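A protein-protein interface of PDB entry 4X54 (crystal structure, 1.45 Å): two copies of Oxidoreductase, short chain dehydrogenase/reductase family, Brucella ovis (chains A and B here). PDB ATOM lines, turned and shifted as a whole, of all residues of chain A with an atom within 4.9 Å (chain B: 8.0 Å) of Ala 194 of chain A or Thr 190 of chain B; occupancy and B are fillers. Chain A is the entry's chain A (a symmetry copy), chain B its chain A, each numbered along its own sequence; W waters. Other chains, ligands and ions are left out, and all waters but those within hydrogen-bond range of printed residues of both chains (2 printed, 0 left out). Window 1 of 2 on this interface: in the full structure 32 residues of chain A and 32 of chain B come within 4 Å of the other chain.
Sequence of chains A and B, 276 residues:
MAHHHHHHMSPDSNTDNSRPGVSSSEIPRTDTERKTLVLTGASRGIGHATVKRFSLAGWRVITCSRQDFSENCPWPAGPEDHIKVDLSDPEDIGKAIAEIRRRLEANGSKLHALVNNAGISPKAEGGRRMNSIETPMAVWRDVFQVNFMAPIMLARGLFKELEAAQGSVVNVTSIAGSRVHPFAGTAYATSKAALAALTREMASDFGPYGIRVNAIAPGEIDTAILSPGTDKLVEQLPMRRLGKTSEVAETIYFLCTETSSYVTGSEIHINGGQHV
The side-chain hydroxyl of Thr 186 of chain B lies within hydrogen-bond range of the side-chain carboxylate of Glu 201 of chain A, 2.7 Å away.
The backbone NH of Ser 132 of chain B sits at hydrogen-bond distance from the side-chain hydroxyl of Thr 186 of chain B (3.2 Å). The indole nitrogen (NE1) of Trp 140 of chain B lies within hydrogen-bond range of the backbone carbonyl oxygen (O) of Thr 135 of chain B (3.0 Å). The side-chain hydroxyl (OG1) of Thr 190 of chain B sits at hydrogen-bond distance from the backbone carbonyl oxygen (O) of Thr 186 of chain B (2.9 Å). The backbone carbonyl oxygen of Ala 187 of chain B is in hydrogen-bond range of the side-chain hydroxyl of Thr 190 of chain B, at 3.2 Å.
Among the printed residues, merely in contact across the chains: Phe 144 of chain A with Phe 144 of chain B (3.6 Å), Phe 144 of chain A with Phe 148 of chain B (3.8 Å), Phe 148 of chain A with Trp 140 of chain B (3.7 Å), Phe 148 of chain A with Phe 144 of chain B (3.8 Å), Phe 148 of chain A with Thr 190 of chain B (3.5 Å), Thr 190 of chain A with Phe 148 of chain B (3.5 Å), Thr 190 of chain A with Ala 194 of chain B (3.96 Å), Thr 190 of chain A with Ala 197 of chain B (3.9 Å), Ala 193 of chain A with Ala 197 of chain B (3.4 Å), Ala 194 of chain A with Thr 190 of chain B (3.96 Å), Ala 197 of chain A with Thr 190 of chain B (3.9 Å), Ala 197 of chain A with Ala 193 of chain B (3.4 Å), Leu 198 of chain A with Trp 140 of chain B (3.9 Å), Leu 198 of chain A with Thr 190 of chain B (3.5 Å) and Glu 201 of chain A with Ala 189 of chain B (3.3 Å).
Of the printed residues of chain B, Ala 194 of chain A touches Thr 190 (3.96 Å). Thr 190 of chain B touches just these residues of chain A: Phe 148, Ala 194, Ala 197 and Leu 198. Ala 193 of chain A touches just one residue of chain B: Ala 197 (3.4 Å). Printed residues of chain A within 4 Å of Phe 148 of chain B: Phe 144 and Thr 190. Printed residues of chain A within 4 Å of Phe 144 of chain B: Phe 144 and Phe 148. Printed residues of chain A within 4 Å of Ala 193 of chain B: Ala 197. Printed residues of chain B within 4 Å of Ala 197 of chain A: Thr 190 (3.9 Å) and Ala 193 (3.4 Å). The nearest residue of chain A that does not touch Thr 190 of chain B is Glu 201 of chain A (4.7 Å).
Printed residues of chain B that touch a printed residue of chain A: Trp 140, Phe 144, Phe 148, Thr 186, Ala 189, Thr 190, Ala 193, Ala 194 and Ala 197. Hydrophobic or aromatic side chains of chain B within 4 Å of the printed part of chain A: Trp 140, Phe 144, Phe 148, Ala 189, Ala 193, Ala 194 and Ala 197. Along chain A the printed residues that touch a printed residue of chain B span positions 144 to 201. Among the printed residues, no Asp or Glu carboxylate lies within 4 Å of a Lys or Arg side-chain nitrogen of the other chain.
Phe 144 of chain B touches its own counterpart, Phe 144 of chain A. Phe 148 of chain A touches Thr 190 of chain B, and with the chains exchanged Thr 190 of chain A touches Phe 148 of chain B. Thr 190 of chain A touches Ala 194 of chain B, and with the chains exchanged Ala 194 of chain A touches Thr 190 of chain B. Thr 190 of chain A touches Ala 197 of chain B, and with the chains exchanged Ala 197 of chain A touches Thr 190 of chain B.
Water W1 bridges the side-chain carboxylate of Glu 201 of chain A and the backbone carbonyl oxygen of Ala 176 of chain B. Water W2 lies within hydrogen-bond range of OE2 of Glu 201 of chain A (2.7 Å) and O of Ala 184 of chain B (2.9 Å).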
ATOM      1  N   PHE A 144       8.063 -27.095 -19.906  1.00  0.00           N
ATOM      2  CA  PHE A 144       7.350 -25.993 -20.582  1.00  0.00           C
ATOM      3  C   PHE A 144       6.043 -25.703 -19.843  1.00  0.00           C
ATOM      4  O   PHE A 144       5.670 -24.517 -19.764  1.00  0.00           O
ATOM      5  CB  PHE A 144       7.081 -26.298 -22.036  1.00  0.00           C
ATOM      6  CG  PHE A 144       8.212 -25.857 -22.918  1.00  0.00           C
ATOM      7  CD1 PHE A 144       9.428 -26.556 -22.964  1.00  0.00           C
ATOM      8  CD2 PHE A 144       8.114 -24.674 -23.652  1.00  0.00           C
ATOM      9  CE1 PHE A 144      10.526 -26.119 -23.752  1.00  0.00           C
ATOM     10  CE2 PHE A 144       9.194 -24.244 -24.454  1.00  0.00           C
ATOM     11  CZ  PHE A 144      10.381 -24.945 -24.504  1.00  0.00           C
ATOM     12  N   PHE A 148       6.636 -21.940 -18.697  1.00  0.00           N
ATOM     13  CA  PHE A 148       6.148 -21.159 -19.823  1.00  0.00           C
ATOM     14  C   PHE A 148       4.623 -21.105 -19.814  1.00  0.00           C
ATOM     15  O   PHE A 148       4.036 -19.987 -19.925  1.00  0.00           O
ATOM     16  CB  PHE A 148       6.689 -21.758 -21.121  1.00  0.00           C
ATOM     17  CG  PHE A 148       6.084 -21.172 -22.390  1.00  0.00           C
ATOM     18  CD1 PHE A 148       6.667 -20.070 -23.027  1.00  0.00           C
ATOM     19  CD2 PHE A 148       4.958 -21.724 -22.986  1.00  0.00           C
ATOM     20  CE1 PHE A 148       6.096 -19.519 -24.157  1.00  0.00           C
ATOM     21  CE2 PHE A 148       4.375 -21.148 -24.157  1.00  0.00           C
ATOM     22  CZ  PHE A 148       4.986 -20.022 -24.724  1.00  0.00           C
ATOM     23  N   THR A 190      15.504 -23.544 -23.226  1.00  0.00           N
ATOM     24  CA  THR A 190      14.536 -23.258 -24.281  1.00  0.00           C
ATOM     25  C   THR A 190      13.201 -22.725 -23.782  1.00  0.00           C
ATOM     26  O   THR A 190      12.617 -21.844 -24.421  1.00  0.00           O
ATOM     27  CB  THR A 190      14.324 -24.517 -25.162  1.00  0.00           C
ATOM     28  OG1 THR A 190      13.850 -25.605 -24.341  1.00  0.00           O
ATOM     29  CG2 THR A 190      15.580 -24.948 -25.924  1.00  0.00           C
ATOM     30  N   SER A 191      12.761 -23.186 -22.610  1.00  0.00           N
ATOM     31  CA  SER A 191      11.506 -22.679 -22.041  1.00  0.00           C
ATOM     32  C   SER A 191      11.709 -21.253 -21.577  1.00  0.00           C
ATOM     33  O   SER A 191      10.768 -20.464 -21.702  1.00  0.00           O
ATOM     34  CB  SER A 191      10.982 -23.587 -20.927  1.00  0.00           C
ATOM     35  OG  SER A 191      11.865 -23.608 -19.840  1.00  0.00           O
ATOM     36  N   LYS A 192      12.895 -20.915 -21.102  1.00  0.00           N
ATOM     37  CA  LYS A 192      13.120 -19.531 -20.691  1.00  0.00           C
ATOM     38  C   LYS A 192      13.233 -18.595 -21.892  1.00  0.00           C
ATOM     39  O   LYS A 192      12.826 -17.421 -21.843  1.00  0.00           O
ATOM     40  CB  LYS A 192      14.379 -19.448 -19.803  1.00  0.00           C
ATOM     41  CG  LYS A 192      14.117 -19.991 -18.351  1.00  0.00           C
ATOM     42  CD  LYS A 192      13.130 -19.112 -17.590  1.00  0.00           C
ATOM     43  CE  LYS A 192      13.193 -19.470 -16.086  1.00  0.00           C
ATOM     44  NZ  LYS A 192      12.134 -18.629 -15.362  1.00  0.00           N
ATOM     45  N   ALA A 193      13.825 -19.075 -22.972  1.00  0.00           N
ATOM     46  CA  ALA A 193      13.833 -18.291 -24.238  1.00  0.00           C
ATOM     47  C   ALA A 193      12.386 -18.092 -24.712  1.00  0.00           C
ATOM     48  O   ALA A 193      12.018 -16.987 -25.134  1.00  0.00           O
ATOM     49  CB  ALA A 193      14.653 -19.013 -25.309  1.00  0.00           C
ATOM     50  N   ALA A 194      11.569 -19.149 -24.630  1.00  0.00           N
ATOM     51  CA  ALA A 194      10.174 -19.009 -25.006  1.00  0.00           C
ATOM     52  C   ALA A 194       9.434 -18.027 -24.058  1.00  0.00           C
ATOM     53  O   ALA A 194       8.603 -17.223 -24.550  1.00  0.00           O
ATOM     54  CB  ALA A 194       9.515 -20.350 -24.960  1.00  0.00           C
ATOM     55  N   LEU A 195       9.783 -18.043 -22.789  1.00  0.00           N
ATOM     56  CA  LEU A 195       9.132 -17.112 -21.845  1.00  0.00           C
ATOM     57  C   LEU A 195       9.501 -15.659 -22.180  1.00  0.00           C
ATOM     58  O   LEU A 195       8.643 -14.775 -22.008  1.00  0.00           O
ATOM     59  CB  LEU A 195       9.600 -17.471 -20.430  1.00  0.00           C
ATOM     60  CG  LEU A 195       8.970 -16.628 -19.308  1.00  0.00           C
ATOM     61  CD1 LEU A 195       7.446 -16.738 -19.268  1.00  0.00           C
ATOM     62  CD2 LEU A 195       9.599 -17.002 -17.935  1.00  0.00           C
ATOM     63  N   ALA A 196      10.737 -15.369 -22.613  1.00  0.00           N
ATOM     64  CA  ALA A 196      11.057 -14.001 -22.974  1.00  0.00           C
ATOM     65  C   ALA A 196      10.173 -13.561 -24.165  1.00  0.00           C
ATOM     66  O   ALA A 196       9.628 -12.442 -24.185  1.00  0.00           O
ATOM     67  CB  ALA A 196      12.544 -13.892 -23.303  1.00  0.00           C
ATOM     68  N   ALA A 197      10.031 -14.426 -25.159  1.00  0.00           N
ATOM     69  CA  ALA A 197       9.156 -14.086 -26.281  1.00  0.00           C
ATOM     70  C   ALA A 197       7.697 -13.974 -25.868  1.00  0.00           C
ATOM     71  O   ALA A 197       7.002 -13.032 -26.333  1.00  0.00           O
ATOM     72  CB  ALA A 197       9.328 -15.161 -27.402  1.00  0.00           C
ATOM     73  N   LEU A 198       7.245 -14.856 -24.976  1.00  0.00           N
ATOM     74  CA  LEU A 198       5.881 -14.710 -24.434  1.00  0.00           C
ATOM     75  C   LEU A 198       5.680 -13.370 -23.743  1.00  0.00           C
ATOM     76  O   LEU A 198       4.606 -12.785 -23.893  1.00  0.00           O
ATOM     77  CB  LEU A 198       5.653 -15.859 -23.472  1.00  0.00           C
ATOM     78  CG  LEU A 198       4.268 -15.911 -22.796  1.00  0.00           C
ATOM     79  CD1 LEU A 198       3.133 -16.094 -23.796  1.00  0.00           C
ATOM     80  CD2 LEU A 198       4.202 -16.980 -21.746  1.00  0.00           C
ATOM     81  N   GLU A 201       5.048 -10.728 -26.357  1.00  0.00           N
ATOM     82  CA  GLU A 201       3.707 -10.889 -26.933  1.00  0.00           C
ATOM     83  C   GLU A 201       2.637 -10.470 -25.930  1.00  0.00           C
ATOM     84  O   GLU A 201       1.703  -9.718 -26.311  1.00  0.00           O
ATOM     85  CB  GLU A 201       3.492 -12.352 -27.370  1.00  0.00           C
ATOM     86  CG  GLU A 201       4.367 -12.701 -28.584  1.00  0.00           C
ATOM     87  CD  GLU A 201       3.701 -12.436 -29.895  1.00  0.00           C
ATOM     88  OE1 GLU A 201       2.432 -12.389 -29.978  1.00  0.00           O
ATOM     89  OE2 GLU A 201       4.394 -12.269 -30.919  1.00  0.00           O
ATOM     90  N   SER B 132      -1.907 -14.137 -27.046  1.00  0.00           N
ATOM     91  CA  SER B 132      -1.583 -14.911 -25.849  1.00  0.00           C
ATOM     92  C   SER B 132      -2.796 -15.141 -24.976  1.00  0.00           C
ATOM     93  O   SER B 132      -2.867 -16.163 -24.273  1.00  0.00           O
ATOM     94  CB  SER B 132      -0.495 -14.208 -25.066  1.00  0.00           C
ATOM     95  OG  SER B 132      -0.991 -13.042 -24.427  1.00  0.00           O
ATOM     96  N   THR B 135      -5.188 -18.065 -27.022  1.00  0.00           N
ATOM     97  CA  THR B 135      -4.682 -19.365 -27.536  1.00  0.00           C
ATOM     98  C   THR B 135      -5.022 -20.488 -26.573  1.00  0.00           C
ATOM     99  O   THR B 135      -4.568 -20.442 -25.432  1.00  0.00           O
ATOM    100  CB  THR B 135      -3.151 -19.297 -27.691  1.00  0.00           C
ATOM    101  OG1 THR B 135      -2.809 -18.294 -28.672  1.00  0.00           O
ATOM    102  CG2 THR B 135      -2.595 -20.606 -28.165  1.00  0.00           C
ATOM    103  N   TRP B 140      -1.323 -24.313 -28.122  1.00  0.00           N
ATOM    104  CA  TRP B 140       0.053 -24.201 -27.659  1.00  0.00           C
ATOM    105  C   TRP B 140       0.768 -25.546 -27.810  1.00  0.00           C
ATOM    106  O   TRP B 140       1.933 -25.618 -28.250  1.00  0.00           O
ATOM    107  CB  TRP B 140       0.091 -23.836 -26.157  1.00  0.00           C
ATOM    108  CG  TRP B 140      -0.412 -22.485 -25.753  1.00  0.00           C
ATOM    109  CD1 TRP B 140      -1.589 -22.232 -25.123  1.00  0.00           C
ATOM    110  CD2 TRP B 140       0.255 -21.199 -25.903  1.00  0.00           C
ATOM    111  NE1 TRP B 140      -1.689 -20.888 -24.857  1.00  0.00           N
ATOM    112  CE2 TRP B 140      -0.590 -20.236 -25.340  1.00  0.00           C
ATOM    113  CE3 TRP B 140       1.471 -20.789 -26.464  1.00  0.00           C
ATOM    114  CZ2 TRP B 140      -0.286 -18.885 -25.304  1.00  0.00           C
ATOM    115  CZ3 TRP B 140       1.750 -19.441 -26.473  1.00  0.00           C
ATOM    116  CH2 TRP B 140       0.885 -18.506 -25.863  1.00  0.00           C
ATOM    117  N   VAL B 143       1.243 -26.526 -31.685  1.00  0.00           N
ATOM    118  CA  VAL B 143       2.219 -25.673 -32.351  1.00  0.00           C
ATOM    119  C   VAL B 143       3.624 -25.919 -31.852  1.00  0.00           C
ATOM    120  O   VAL B 143       4.543 -25.986 -32.652  1.00  0.00           O
ATOM    121  CB  VAL B 143       1.802 -24.196 -32.154  1.00  0.00           C
ATOM    122  CG1 VAL B 143       2.921 -23.240 -32.727  1.00  0.00           C
ATOM    123  CG2 VAL B 143       0.488 -23.890 -32.826  1.00  0.00           C
ATOM    124  N   PHE B 144       3.809 -26.124 -30.557  1.00  0.00           N
ATOM    125  CA  PHE B 144       5.161 -26.458 -30.067  1.00  0.00           C
ATOM    126  C   PHE B 144       5.541 -27.863 -30.537  1.00  0.00           C
ATOM    127  O   PHE B 144       6.729 -28.070 -30.852  1.00  0.00           O
ATOM    128  CB  PHE B 144       5.260 -26.358 -28.564  1.00  0.00           C
ATOM    129  CG  PHE B 144       5.645 -24.976 -28.121  1.00  0.00           C
ATOM    130  CD1 PHE B 144       4.737 -23.907 -28.164  1.00  0.00           C
ATOM    131  CD2 PHE B 144       6.958 -24.698 -27.739  1.00  0.00           C
ATOM    132  CE1 PHE B 144       5.104 -22.584 -27.800  1.00  0.00           C
ATOM    133  CE2 PHE B 144       7.325 -23.390 -27.357  1.00  0.00           C
ATOM    134  CZ  PHE B 144       6.421 -22.347 -27.389  1.00  0.00           C
ATOM    135  N   ASN B 147       6.484 -27.244 -34.324  1.00  0.00           N
ATOM    136  CA  ASN B 147       7.500 -26.237 -34.665  1.00  0.00           C
ATOM    137  C   ASN B 147       8.799 -26.433 -33.948  1.00  0.00           C
ATOM    138  O   ASN B 147       9.833 -25.906 -34.401  1.00  0.00           O
ATOM    139  CB  ASN B 147       6.944 -24.820 -34.352  1.00  0.00           C
ATOM    140  CG  ASN B 147       5.798 -24.397 -35.239  1.00  0.00           C
ATOM    141  OD1 ASN B 147       5.266 -25.170 -36.040  1.00  0.00           O
ATOM    142  ND2 ASN B 147       5.350 -23.153 -35.029  1.00  0.00           N
ATOM    143  N   PHE B 148       8.731 -27.078 -32.779  1.00  0.00           N
ATOM    144  CA  PHE B 148       9.833 -27.120 -31.832  1.00  0.00           C
ATOM    145  C   PHE B 148      10.202 -28.565 -31.505  1.00  0.00           C
ATOM    146  O   PHE B 148      11.413 -28.932 -31.575  1.00  0.00           O
ATOM    147  CB  PHE B 148       9.448 -26.333 -30.579  1.00  0.00           C
ATOM    148  CG  PHE B 148      10.423 -26.476 -29.417  1.00  0.00           C
ATOM    149  CD1 PHE B 148      11.495 -25.588 -29.260  1.00  0.00           C
ATOM    150  CD2 PHE B 148      10.270 -27.461 -28.450  1.00  0.00           C
ATOM    151  CE1 PHE B 148      12.397 -25.741 -28.225  1.00  0.00           C
ATOM    152  CE2 PHE B 148      11.209 -27.610 -27.382  1.00  0.00           C
ATOM    153  CZ  PHE B 148      12.281 -26.713 -27.303  1.00  0.00           C
ATOM    154  N   ALA B 176       9.454 -13.495 -36.393  1.00  0.00           N
ATOM    155  CA  ALA B 176       8.437 -13.445 -35.294  1.00  0.00           C
ATOM    156  C   ALA B 176       9.047 -13.922 -34.000  1.00  0.00           C
ATOM    157  O   ALA B 176       8.502 -13.651 -32.932  1.00  0.00           O
ATOM    158  CB  ALA B 176       7.201 -14.268 -35.647  1.00  0.00           C
ATOM    159  N   GLY B 177      10.150 -14.664 -34.059  1.00  0.00           N
ATOM    160  CA  GLY B 177      10.760 -15.160 -32.833  1.00  0.00           C
ATOM    161  C   GLY B 177      11.405 -14.008 -32.050  1.00  0.00           C
ATOM    162  O   GLY B 177      11.689 -14.196 -30.863  1.00  0.00           O
ATOM    163  N   SER B 178      11.631 -12.868 -32.670  1.00  0.00           N
ATOM    164  CA  SER B 178      12.227 -11.753 -31.938  1.00  0.00           C
ATOM    165  C   SER B 178      11.440 -10.454 -32.007  1.00  0.00           C
ATOM    166  O   SER B 178      11.853  -9.497 -31.363  1.00  0.00           O
ATOM    167  CB  SER B 178      13.666 -11.560 -32.421  1.00  0.00           C
ATOM    168  OG  SER B 178      13.743 -11.272 -33.807  1.00  0.00           O
ATOM    169  N   ALA B 184       1.750 -13.396 -37.594  1.00  0.00           N
ATOM    170  CA  ALA B 184       2.135 -14.598 -36.879  1.00  0.00           C
ATOM    171  C   ALA B 184       1.576 -14.526 -35.480  1.00  0.00           C
ATOM    172  O   ALA B 184       1.832 -13.570 -34.765  1.00  0.00           O
ATOM    173  CB  ALA B 184       3.666 -14.724 -36.827  1.00  0.00           C
ATOM    174  N   GLY B 185       0.831 -15.545 -35.081  1.00  0.00           N
ATOM    175  CA  GLY B 185       0.282 -15.579 -33.737  1.00  0.00           C
ATOM    176  C   GLY B 185       1.307 -15.845 -32.657  1.00  0.00           C
ATOM    177  O   GLY B 185       2.458 -16.140 -32.919  1.00  0.00           O
ATOM    178  N   THR B 186       0.846 -15.761 -31.416  1.00  0.00           N
ATOM    179  CA  THR B 186       1.744 -15.891 -30.295  1.00  0.00           C
ATOM    180  C   THR B 186       2.337 -17.288 -30.162  1.00  0.00           C
ATOM    181  O   THR B 186       3.530 -17.420 -29.824  1.00  0.00           O
ATOM    182  CB  THR B 186       1.000 -15.508 -29.023  1.00  0.00           C
ATOM    183  OG1 THR B 186       0.528 -14.178 -29.149  1.00  0.00           O
ATOM    184  CG2 THR B 186       1.958 -15.624 -27.805  1.00  0.00           C
ATOM    185  N   ALA B 187       1.579 -18.347 -30.440  1.00  0.00           N
ATOM    186  CA  ALA B 187       2.164 -19.680 -30.331  1.00  0.00           C
ATOM    187  C   ALA B 187       3.285 -19.853 -31.376  1.00  0.00           C
ATOM    188  O   ALA B 187       4.339 -20.422 -31.050  1.00  0.00           O
ATOM    189  CB  ALA B 187       1.062 -20.704 -30.524  1.00  0.00           C
ATOM    190  N   TYR B 188       3.078 -19.321 -32.587  1.00  0.00           N
ATOM    191  CA  TYR B 188       4.154 -19.385 -33.580  1.00  0.00           C
ATOM    192  C   TYR B 188       5.374 -18.601 -33.135  1.00  0.00           C
ATOM    193  O   TYR B 188       6.486 -19.104 -33.218  1.00  0.00           O
ATOM    194  CB  TYR B 188       3.627 -18.870 -34.902  1.00  0.00           C
ATOM    195  CG  TYR B 188       4.632 -18.916 -36.047  1.00  0.00           C
ATOM    196  CD1 TYR B 188       4.735 -20.078 -36.823  1.00  0.00           C
ATOM    197  CD2 TYR B 188       5.440 -17.815 -36.351  1.00  0.00           C
ATOM    198  CE1 TYR B 188       5.609 -20.092 -37.894  1.00  0.00           C
ATOM    199  CE2 TYR B 188       6.341 -17.849 -37.403  1.00  0.00           C
ATOM    200  CZ  TYR B 188       6.400 -18.988 -38.165  1.00  0.00           C
ATOM    201  OH  TYR B 188       7.224 -19.017 -39.288  1.00  0.00           O
ATOM    202  N   ALA B 189       5.184 -17.366 -32.692  1.00  0.00           N
ATOM    203  CA  ALA B 189       6.305 -16.528 -32.267  1.00  0.00           C
ATOM    204  C   ALA B 189       7.108 -17.183 -31.183  1.00  0.00           C
ATOM    205  O   ALA B 189       8.376 -17.200 -31.224  1.00  0.00           O
ATOM    206  CB  ALA B 189       5.762 -15.198 -31.786  1.00  0.00           C
ATOM    207  N   THR B 190       6.390 -17.629 -30.142  1.00  0.00           N
ATOM    208  CA  THR B 190       7.105 -18.218 -29.013  1.00  0.00           C
ATOM    209  C   THR B 190       7.777 -19.548 -29.321  1.00  0.00           C
ATOM    210  O   THR B 190       8.883 -19.802 -28.833  1.00  0.00           O
ATOM    211  CB  THR B 190       6.154 -18.356 -27.796  1.00  0.00           C
ATOM    212  OG1 THR B 190       5.032 -19.188 -28.154  1.00  0.00           O
ATOM    213  CG2 THR B 190       5.657 -17.013 -27.253  1.00  0.00           C
ATOM    214  N   SER B 191       7.162 -20.355 -30.187  1.00  0.00           N
ATOM    215  CA  SER B 191       7.776 -21.632 -30.570  1.00  0.00           C
ATOM    216  C   SER B 191       8.983 -21.363 -31.443  1.00  0.00           C
ATOM    217  O   SER B 191       9.959 -22.112 -31.327  1.00  0.00           O
ATOM    218  CB  SER B 191       6.767 -22.567 -31.240  1.00  0.00           C
ATOM    219  OG  SER B 191       6.314 -22.030 -32.451  1.00  0.00           O
ATOM    220  N   LYS B 192       8.947 -20.319 -32.251  1.00  0.00           N
ATOM    221  CA  LYS B 192      10.122 -20.021 -33.067  1.00  0.00           C
ATOM    222  C   LYS B 192      11.263 -19.448 -32.230  1.00  0.00           C
ATOM    223  O   LYS B 192      12.453 -19.682 -32.506  1.00  0.00           O
ATOM    224  CB  LYS B 192       9.734 -19.056 -34.208  1.00  0.00           C
ATOM    225  CG  LYS B 192       8.940 -19.783 -35.354  1.00  0.00           C
ATOM    226  CD  LYS B 192       9.808 -20.806 -36.081  1.00  0.00           C
ATOM    227  CE  LYS B 192       9.110 -21.211 -37.401  1.00  0.00           C
ATOM    228  NZ  LYS B 192       9.965 -22.297 -38.065  1.00  0.00           N
ATOM    229  N   ALA B 193      10.930 -18.656 -31.225  1.00  0.00           N
ATOM    230  CA  ALA B 193      11.965 -18.189 -30.261  1.00  0.00           C
ATOM    231  C   ALA B 193      12.565 -19.405 -29.542  1.00  0.00           C
ATOM    232  O   ALA B 193      13.789 -19.481 -29.367  1.00  0.00           O
ATOM    233  CB  ALA B 193      11.352 -17.217 -29.250  1.00  0.00           C
ATOM    234  N   ALA B 194      11.712 -20.356 -29.139  1.00  0.00           N
ATOM    235  CA  ALA B 194      12.224 -21.558 -28.508  1.00  0.00           C
ATOM    236  C   ALA B 194      13.095 -22.382 -29.494  1.00  0.00           C
ATOM    237  O   ALA B 194      14.146 -22.922 -29.065  1.00  0.00           O
ATOM    238  CB  ALA B 194      11.075 -22.388 -28.030  1.00  0.00           C
ATOM    239  N   LEU B 195      12.716 -22.402 -30.754  1.00  0.00           N
ATOM    240  CA  LEU B 195      13.520 -23.149 -31.742  1.00  0.00           C
ATOM    241  C   LEU B 195      14.901 -22.498 -31.915  1.00  0.00           C
ATOM    242  O   LEU B 195      15.882 -23.235 -32.122  1.00  0.00           O
ATOM    243  CB  LEU B 195      12.756 -23.145 -33.071  1.00  0.00           C
ATOM    244  CG  LEU B 195      13.432 -23.932 -34.207  1.00  0.00           C
ATOM    245  CD1 LEU B 195      13.637 -25.408 -33.865  1.00  0.00           C
ATOM    246  CD2 LEU B 195      12.631 -23.766 -35.530  1.00  0.00           C
ATOM    247  N   ALA B 196      15.018 -21.163 -31.874  1.00  0.00           N
ATOM    248  CA  ALA B 196      16.334 -20.563 -31.986  1.00  0.00           C
ATOM    249  C   ALA B 196      17.210 -21.013 -30.793  1.00  0.00           C
ATOM    250  O   ALA B 196      18.393 -21.365 -30.958  1.00  0.00           O
ATOM    251  CB  ALA B 196      16.201 -19.044 -32.050  1.00  0.00           C
ATOM    252  N   ALA B 197      16.646 -20.998 -29.594  1.00  0.00           N
ATOM    253  CA  ALA B 197      17.408 -21.471 -28.441  1.00  0.00           C
ATOM    254  C   ALA B 197      17.726 -22.957 -28.523  1.00  0.00           C
ATOM    255  O   ALA B 197      18.873 -23.354 -28.189  1.00  0.00           O
ATOM    256  CB  ALA B 197      16.607 -21.153 -27.137  1.00  0.00           C
HETATM  257  O   HOH W   1       7.070 -11.961 -31.099  1.00  0.00           O
HETATM  258  O   HOH W   2       4.192 -12.405 -33.638  1.00  0.00           O
